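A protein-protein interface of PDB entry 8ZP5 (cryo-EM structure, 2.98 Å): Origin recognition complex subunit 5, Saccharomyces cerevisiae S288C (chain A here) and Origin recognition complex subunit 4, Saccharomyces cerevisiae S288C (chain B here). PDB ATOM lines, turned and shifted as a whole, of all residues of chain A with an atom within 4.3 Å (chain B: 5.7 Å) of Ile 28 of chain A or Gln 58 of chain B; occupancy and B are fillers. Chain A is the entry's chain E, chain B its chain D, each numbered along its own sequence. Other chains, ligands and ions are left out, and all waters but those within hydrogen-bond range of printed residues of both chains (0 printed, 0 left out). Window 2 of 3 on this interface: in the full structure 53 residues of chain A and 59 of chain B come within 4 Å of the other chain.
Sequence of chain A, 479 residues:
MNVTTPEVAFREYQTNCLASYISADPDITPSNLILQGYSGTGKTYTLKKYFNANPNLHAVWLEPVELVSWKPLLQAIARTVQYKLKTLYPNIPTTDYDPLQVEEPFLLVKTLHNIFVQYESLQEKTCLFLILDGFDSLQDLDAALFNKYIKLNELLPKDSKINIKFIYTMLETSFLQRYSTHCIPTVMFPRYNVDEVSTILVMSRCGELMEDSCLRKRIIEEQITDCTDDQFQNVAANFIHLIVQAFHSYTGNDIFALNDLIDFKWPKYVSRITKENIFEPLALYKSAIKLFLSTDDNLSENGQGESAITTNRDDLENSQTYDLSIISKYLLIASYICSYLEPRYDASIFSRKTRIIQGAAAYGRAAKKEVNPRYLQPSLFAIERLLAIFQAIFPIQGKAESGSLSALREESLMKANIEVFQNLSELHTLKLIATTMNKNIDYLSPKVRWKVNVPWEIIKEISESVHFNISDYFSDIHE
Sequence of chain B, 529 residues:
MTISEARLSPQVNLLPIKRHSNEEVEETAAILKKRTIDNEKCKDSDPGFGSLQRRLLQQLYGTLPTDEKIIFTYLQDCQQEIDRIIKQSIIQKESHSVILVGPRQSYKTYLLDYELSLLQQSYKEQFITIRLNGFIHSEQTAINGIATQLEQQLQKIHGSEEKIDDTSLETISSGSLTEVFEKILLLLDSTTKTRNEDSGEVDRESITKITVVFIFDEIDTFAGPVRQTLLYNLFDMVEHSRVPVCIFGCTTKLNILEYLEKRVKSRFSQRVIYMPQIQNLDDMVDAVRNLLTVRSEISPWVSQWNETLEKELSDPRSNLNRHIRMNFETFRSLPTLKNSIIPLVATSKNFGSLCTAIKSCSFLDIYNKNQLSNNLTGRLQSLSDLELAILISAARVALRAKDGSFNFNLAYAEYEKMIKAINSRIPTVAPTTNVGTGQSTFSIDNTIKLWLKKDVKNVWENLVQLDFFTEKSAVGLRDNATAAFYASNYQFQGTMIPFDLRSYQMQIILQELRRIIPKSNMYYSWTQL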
ATOM      1  N   TYR A  21      22.231  -5.958  -4.777  1.00  0.00           N
ATOM      2  CA  TYR A  21      22.172  -7.032  -5.760  1.00  0.00           C
ATOM      3  C   TYR A  21      23.160  -6.828  -6.904  1.00  0.00           C
ATOM      4  O   TYR A  21      23.879  -7.760  -7.276  1.00  0.00           O
ATOM      5  CB  TYR A  21      20.749  -7.167  -6.308  1.00  0.00           C
ATOM      6  CG  TYR A  21      19.743  -7.648  -5.288  1.00  0.00           C
ATOM      7  CD1 TYR A  21      19.921  -8.852  -4.626  1.00  0.00           C
ATOM      8  CD2 TYR A  21      18.614  -6.901  -4.991  1.00  0.00           C
ATOM      9  CE1 TYR A  21      19.005  -9.297  -3.695  1.00  0.00           C
ATOM     10  CE2 TYR A  21      17.694  -7.335  -4.062  1.00  0.00           C
ATOM     11  CZ  TYR A  21      17.894  -8.534  -3.418  1.00  0.00           C
ATOM     12  OH  TYR A  21      16.977  -8.971  -2.492  1.00  0.00           O
ATOM     13  N   SER A  23      26.378  -5.934  -8.258  1.00  0.00           N
ATOM     14  CA  SER A  23      27.764  -5.719  -7.873  1.00  0.00           C
ATOM     15  C   SER A  23      28.671  -6.281  -8.959  1.00  0.00           C
ATOM     16  O   SER A  23      28.277  -7.154  -9.735  1.00  0.00           O
ATOM     17  CB  SER A  23      28.083  -6.364  -6.518  1.00  0.00           C
ATOM     18  OG  SER A  23      28.464  -7.719  -6.676  1.00  0.00           O
ATOM     19  N   ASP A  25      31.140  -8.194  -8.686  1.00  0.00           N
ATOM     20  CA  ASP A  25      31.615  -9.547  -8.430  1.00  0.00           C
ATOM     21  C   ASP A  25      30.565 -10.549  -8.888  1.00  0.00           C
ATOM     22  O   ASP A  25      29.457 -10.556  -8.338  1.00  0.00           O
ATOM     23  CB  ASP A  25      31.908  -9.739  -6.952  1.00  0.00           C
ATOM     24  CG  ASP A  25      32.820 -10.917  -6.685  1.00  0.00           C
ATOM     25  OD1 ASP A  25      33.200 -11.611  -7.650  1.00  0.00           O
ATOM     26  OD2 ASP A  25      33.159 -11.150  -5.507  1.00  0.00           O
ATOM     27  N   PRO A  26      30.858 -11.399  -9.874  1.00  0.00           N
ATOM     28  CA  PRO A  26      29.839 -12.347 -10.352  1.00  0.00           C
ATOM     29  C   PRO A  26      29.407 -13.364  -9.311  1.00  0.00           C
ATOM     30  O   PRO A  26      28.338 -13.966  -9.466  1.00  0.00           O
ATOM     31  CB  PRO A  26      30.524 -13.028 -11.546  1.00  0.00           C
ATOM     32  CG  PRO A  26      31.644 -12.115 -11.927  1.00  0.00           C
ATOM     33  CD  PRO A  26      32.101 -11.486 -10.654  1.00  0.00           C
ATOM     34  N   ASP A  27      30.202 -13.583  -8.264  1.00  0.00           N
ATOM     35  CA  ASP A  27      29.858 -14.589  -7.267  1.00  0.00           C
ATOM     36  C   ASP A  27      28.740 -14.134  -6.339  1.00  0.00           C
ATOM     37  O   ASP A  27      27.995 -14.971  -5.821  1.00  0.00           O
ATOM     38  CB  ASP A  27      31.095 -14.958  -6.446  1.00  0.00           C
ATOM     39  CG  ASP A  27      32.262 -15.382  -7.311  1.00  0.00           C
ATOM     40  OD1 ASP A  27      32.073 -16.262  -8.177  1.00  0.00           O
ATOM     41  OD2 ASP A  27      33.369 -14.834  -7.128  1.00  0.00           O
ATOM     42  N   ILE A  28      28.605 -12.828  -6.114  1.00  0.00           N
ATOM     43  CA  ILE A  28      27.654 -12.322  -5.131  1.00  0.00           C
ATOM     44  C   ILE A  28      26.608 -11.437  -5.794  1.00  0.00           C
ATOM     45  O   ILE A  28      26.081 -10.509  -5.171  1.00  0.00           O
ATOM     46  CB  ILE A  28      28.378 -11.566  -4.003  1.00  0.00           C
ATOM     47  CG1 ILE A  28      29.228 -10.435  -4.576  1.00  0.00           C
ATOM     48  CG2 ILE A  28      29.242 -12.517  -3.196  1.00  0.00           C
ATOM     49  CD1 ILE A  28      29.847  -9.551  -3.521  1.00  0.00           C
ATOM     50  N   THR A  29      26.295 -11.714  -7.058  1.00  0.00           N
ATOM     51  CA  THR A  29      25.201 -11.031  -7.726  1.00  0.00           C
ATOM     52  C   THR A  29      24.261 -12.060  -8.340  1.00  0.00           C
ATOM     53  O   THR A  29      24.717 -13.071  -8.888  1.00  0.00           O
ATOM     54  CB  THR A  29      25.712 -10.062  -8.806  1.00  0.00           C
ATOM     55  OG1 THR A  29      24.601  -9.494  -9.511  1.00  0.00           O
ATOM     56  CG2 THR A  29      26.615 -10.770  -9.790  1.00  0.00           C
ATOM     57  N   GLN B  53      31.576  -9.923   5.176  1.00  0.00           N
ATOM     58  CA  GLN B  53      30.343  -9.670   4.440  1.00  0.00           C
ATOM     59  C   GLN B  53      30.357 -10.359   3.083  1.00  0.00           C
ATOM     60  O   GLN B  53      29.343 -10.924   2.658  1.00  0.00           O
ATOM     61  CB  GLN B  53      30.139  -8.166   4.282  1.00  0.00           C
ATOM     62  CG  GLN B  53      28.943  -7.772   3.446  1.00  0.00           C
ATOM     63  CD  GLN B  53      28.765  -6.270   3.376  1.00  0.00           C
ATOM     64  OE1 GLN B  53      27.973  -5.762   2.587  1.00  0.00           O
ATOM     65  NE2 GLN B  53      29.503  -5.550   4.210  1.00  0.00           N
ATOM     66  N   ARG B  54      31.495 -10.320   2.386  1.00  0.00           N
ATOM     67  CA  ARG B  54      31.595 -11.016   1.107  1.00  0.00           C
ATOM     68  C   ARG B  54      31.437 -12.520   1.288  1.00  0.00           C
ATOM     69  O   ARG B  54      30.769 -13.182   0.484  1.00  0.00           O
ATOM     70  CB  ARG B  54      32.928 -10.690   0.436  1.00  0.00           C
ATOM     71  CG  ARG B  54      32.831 -10.528  -1.068  1.00  0.00           C
ATOM     72  CD  ARG B  54      34.201 -10.314  -1.682  1.00  0.00           C
ATOM     73  NE  ARG B  54      34.963 -11.554  -1.745  1.00  0.00           N
ATOM     74  CZ  ARG B  54      34.822 -12.475  -2.689  1.00  0.00           C
ATOM     75  NH1 ARG B  54      33.952 -12.326  -3.674  1.00  0.00           N
ATOM     76  NH2 ARG B  54      35.572 -13.571  -2.643  1.00  0.00           N
ATOM     77  N   ARG B  55      32.041 -13.076   2.341  1.00  0.00           N
ATOM     78  CA  ARG B  55      31.886 -14.501   2.613  1.00  0.00           C
ATOM     79  C   ARG B  55      30.438 -14.853   2.915  1.00  0.00           C
ATOM     80  O   ARG B  55      29.928 -15.872   2.439  1.00  0.00           O
ATOM     81  CB  ARG B  55      32.786 -14.917   3.773  1.00  0.00           C
ATOM     82  CG  ARG B  55      32.541 -16.332   4.261  1.00  0.00           C
ATOM     83  CD  ARG B  55      32.867 -17.344   3.180  1.00  0.00           C
ATOM     84  NE  ARG B  55      32.604 -18.710   3.615  1.00  0.00           N
ATOM     85  CZ  ARG B  55      33.537 -19.640   3.763  1.00  0.00           C
ATOM     86  NH1 ARG B  55      34.811 -19.388   3.514  1.00  0.00           N
ATOM     87  NH2 ARG B  55      33.182 -20.855   4.169  1.00  0.00           N
ATOM     88  N   LEU B  56      29.758 -14.022   3.708  1.00  0.00           N
ATOM     89  CA  LEU B  56      28.354 -14.277   4.012  1.00  0.00           C
ATOM     90  C   LEU B  56      27.499 -14.224   2.753  1.00  0.00           C
ATOM     91  O   LEU B  56      26.618 -15.070   2.553  1.00  0.00           O
ATOM     92  CB  LEU B  56      27.852 -13.267   5.042  1.00  0.00           C
ATOM     93  CG  LEU B  56      28.119 -13.594   6.510  1.00  0.00           C
ATOM     94  CD1 LEU B  56      27.529 -12.519   7.402  1.00  0.00           C
ATOM     95  CD2 LEU B  56      27.549 -14.955   6.856  1.00  0.00           C
ATOM     96  N   LEU B  57      27.746 -13.237   1.891  1.00  0.00           N
ATOM     97  CA  LEU B  57      26.958 -13.112   0.670  1.00  0.00           C
ATOM     98  C   LEU B  57      27.201 -14.279  -0.277  1.00  0.00           C
ATOM     99  O   LEU B  57      26.261 -14.783  -0.899  1.00  0.00           O
ATOM    100  CB  LEU B  57      27.263 -11.786  -0.016  1.00  0.00           C
ATOM    101  CG  LEU B  57      26.564 -10.599   0.639  1.00  0.00           C
ATOM    102  CD1 LEU B  57      27.381  -9.348   0.444  1.00  0.00           C
ATOM    103  CD2 LEU B  57      25.173 -10.425   0.070  1.00  0.00           C
ATOM    104  N   GLN B  58      28.449 -14.729  -0.405  1.00  0.00           N
ATOM    105  CA  GLN B  58      28.712 -15.867  -1.273  1.00  0.00           C
ATOM    106  C   GLN B  58      28.319 -17.194  -0.640  1.00  0.00           C
ATOM    107  O   GLN B  58      28.207 -18.193  -1.356  1.00  0.00           O
ATOM    108  CB  GLN B  58      30.185 -15.895  -1.688  1.00  0.00           C
ATOM    109  CG  GLN B  58      31.115 -16.568  -0.707  1.00  0.00           C
ATOM    110  CD  GLN B  58      32.560 -16.491  -1.153  1.00  0.00           C
ATOM    111  OE1 GLN B  58      32.943 -15.584  -1.891  1.00  0.00           O
ATOM    112  NE2 GLN B  58      33.370 -17.443  -0.708  1.00  0.00           N
ATOM    113  N   GLN B  59      28.110 -17.231   0.677  1.00  0.00           N
ATOM    114  CA  GLN B  59      27.471 -18.392   1.288  1.00  0.00           C
ATOM    115  C   GLN B  59      25.979 -18.405   0.991  1.00  0.00           C
ATOM    116  O   GLN B  59      25.406 -19.463   0.704  1.00  0.00           O
ATOM    117  CB  GLN B  59      27.709 -18.393   2.796  1.00  0.00           C
ATOM    118  CG  GLN B  59      29.008 -19.032   3.235  1.00  0.00           C
ATOM    119  CD  GLN B  59      29.049 -19.275   4.728  1.00  0.00           C
ATOM    120  OE1 GLN B  59      28.770 -18.378   5.520  1.00  0.00           O
ATOM    121  NE2 GLN B  59      29.393 -20.495   5.120  1.00  0.00           N
ATOM    122  N   LEU B  60      25.335 -17.239   1.066  1.00  0.00           N
ATOM    123  CA  LEU B  60      23.912 -17.155   0.754  1.00  0.00           C
ATOM    124  C   LEU B  60      23.648 -17.464  -0.714  1.00  0.00           C
ATOM    125  O   LEU B  60      22.666 -18.137  -1.045  1.00  0.00           O
ATOM    126  CB  LEU B  60      23.374 -15.773   1.118  1.00  0.00           C
ATOM    127  CG  LEU B  60      23.267 -15.481   2.613  1.00  0.00           C
ATOM    128  CD1 LEU B  60      23.432 -13.999   2.878  1.00  0.00           C
ATOM    129  CD2 LEU B  60      21.942 -15.978   3.155  1.00  0.00           C
ATOM    130  N   TYR B  61      24.508 -16.978  -1.609  1.00  0.00           N
ATOM    131  CA  TYR B  61      24.352 -17.264  -3.029  1.00  0.00           C
ATOM    132  C   TYR B  61      24.820 -18.664  -3.399  1.00  0.00           C
ATOM    133  O   TYR B  61      24.471 -19.154  -4.477  1.00  0.00           O
ATOM    134  CB  TYR B  61      25.110 -16.230  -3.862  1.00  0.00           C
ATOM    135  CG  TYR B  61      24.356 -14.936  -4.046  1.00  0.00           C
ATOM    136  CD1 TYR B  61      23.274 -14.858  -4.909  1.00  0.00           C
ATOM    137  CD2 TYR B  61      24.720 -13.795  -3.351  1.00  0.00           C
ATOM    138  CE1 TYR B  61      22.580 -13.679  -5.076  1.00  0.00           C
ATOM    139  CE2 TYR B  61      24.033 -12.613  -3.510  1.00  0.00           C
ATOM    140  CZ  TYR B  61      22.965 -12.559  -4.374  1.00  0.00           C
ATOM    141  OH  TYR B  61      22.281 -11.378  -4.532  1.00  0.00           O
ATOM    142  N   GLY B  62      25.594 -19.315  -2.536  1.00  0.00           N
ATOM    143  CA  GLY B  62      26.066 -20.654  -2.815  1.00  0.00           C
ATOM    144  C   GLY B  62      27.207 -20.740  -3.799  1.00  0.00           C
ATOM    145  O   GLY B  62      27.455 -21.819  -4.346  1.00  0.00           O
ATOM    146  N   THR B  63      27.913 -19.637  -4.048  1.00  0.00           N
ATOM    147  CA  THR B  63      29.027 -19.620  -4.983  1.00  0.00           C
ATOM    148  C   THR B  63      30.370 -19.859  -4.303  1.00  0.00           C
ATOM    149  O   THR B  63      31.411 -19.501  -4.864  1.00  0.00           O
ATOM    150  CB  THR B  63      29.058 -18.296  -5.748  1.00  0.00           C
ATOM    151  OG1 THR B  63      29.029 -17.205  -4.822  1.00  0.00           O
ATOM    152  CG2 THR B  63      27.862 -18.195  -6.681  1.00  0.00           C
ATOM    153  N   LEU B  64      30.368 -20.447  -3.115  1.00  0.00           N
ATOM    154  CA  LEU B  64      31.601 -20.810  -2.441  1.00  0.00           C
ATOM    155  C   LEU B  64      32.149 -22.110  -3.026  1.00  0.00           C
ATOM    156  O   LEU B  64      31.411 -22.874  -3.653  1.00  0.00           O
ATOM    157  CB  LEU B  64      31.357 -20.930  -0.937  1.00  0.00           C
ATOM    158  CG  LEU B  64      30.647 -22.140  -0.329  1.00  0.00           C
ATOM    159  CD1 LEU B  64      30.809 -22.106   1.178  1.00  0.00           C
ATOM    160  CD2 LEU B  64      29.175 -22.174  -0.697  1.00  0.00           C
ATOM    161  N   PRO B  65      33.448 -22.376  -2.855  1.00  0.00           N
ATOM    162  CA  PRO B  65      34.056 -23.534  -3.524  1.00  0.00           C
ATOM    163  C   PRO B  65      33.389 -24.845  -3.136  1.00  0.00           C
ATOM    164  O   PRO B  65      32.914 -25.021  -2.012  1.00  0.00           O
ATOM    165  CB  PRO B  65      35.513 -23.491  -3.049  1.00  0.00           C
ATOM    166  CG  PRO B  65      35.752 -22.063  -2.728  1.00  0.00           C
ATOM    167  CD  PRO B  65      34.460 -21.561  -2.159  1.00  0.00           C
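O of Asp 27 of chain A lies within hydrogen-bond range of OG1 of Thr 63 of chain B. The side-chain carboxylate (OD2) of Asp 25 of chain A sits close to the guanidinium group (NH1) of Arg 54 of chain B (2.3 Å).
OG1 of Thr 29 of chain A is in hydrogen-bond range of O of Tyr 21 of chain A (2.9 Å). The side-chain hydroxyl (OG) of Ser 23 of chain A lies close to the backbone NH (N) of Asp 25 of chain A, 3.4 Å away. The guanidinium group of Arg 54 of chain B is in hydrogen-bond range of the side-chain amide oxygen of Gln 58 of chain B. The backbone NH (N) of Thr 63 of chain B is in hydrogen-bond range of the backbone carbonyl oxygen (O) of Gln 58 of chain B, at 3.1 Å.
Of the printed residues of chain B, Ile 28 of chain A touches Arg 54, Leu 57, Gln 58 and Tyr 61. Of the printed residues of chain B, Tyr 21 of chain A touches Tyr 61. Of the printed residues of chain B, Asp 27 of chain A touches Tyr 61 and Thr 63. Of the printed residues of chain A, Thr 63 of chain B touches Asp 27. Gln 53 of chain B touches none of the printed residues of chain A. Thr 29 of chain A touches none of the printed residues of chain B. The nearest printed residue of chain A that does not touch Gln 58 of chain B is Asp 27 of chain A (4.7 Å). The nearest printed residue of chain A that does not touch Thr 63 of chain B is Ile 28 of chain A (4.6 Å).
Of the 7 printed residues of chain A, 4 touch a printed residue of chain B. Printed residues of chain A that touch a printed residue of chain B: Tyr 21, Asp 25, Asp 27 and Ile 28. Hydrophobic or aromatic side chains of chain A within 4 Å of the printed part of chain B: Tyr 21 and Ile 28. Of the 13 printed residues of chain B, 5 touch a printed residue of chain A. Among the printed residues, 8 pairs touch across the chains.
Tyr 21 of chain A touches Tyr 61 of chain B (CD1 to OH, 3.5 Å). Asp 27 of chain A touches Tyr 61 of chain B (O to CB, 3.7 Å). Ile 28 of chain A touches Arg 54 of chain B (CD1 to CG, 3.98 Å). CG2 of Ile 28 of chain A touches CB of Leu 57 of chain B (3.8 Å). CG2 of Ile 28 of chain A touches N of Gln 58 of chain B, 3.6 Å away. Tyr 61 of chain B touches Ile 28 of chain A (CE2 to O, 3.4 Å).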
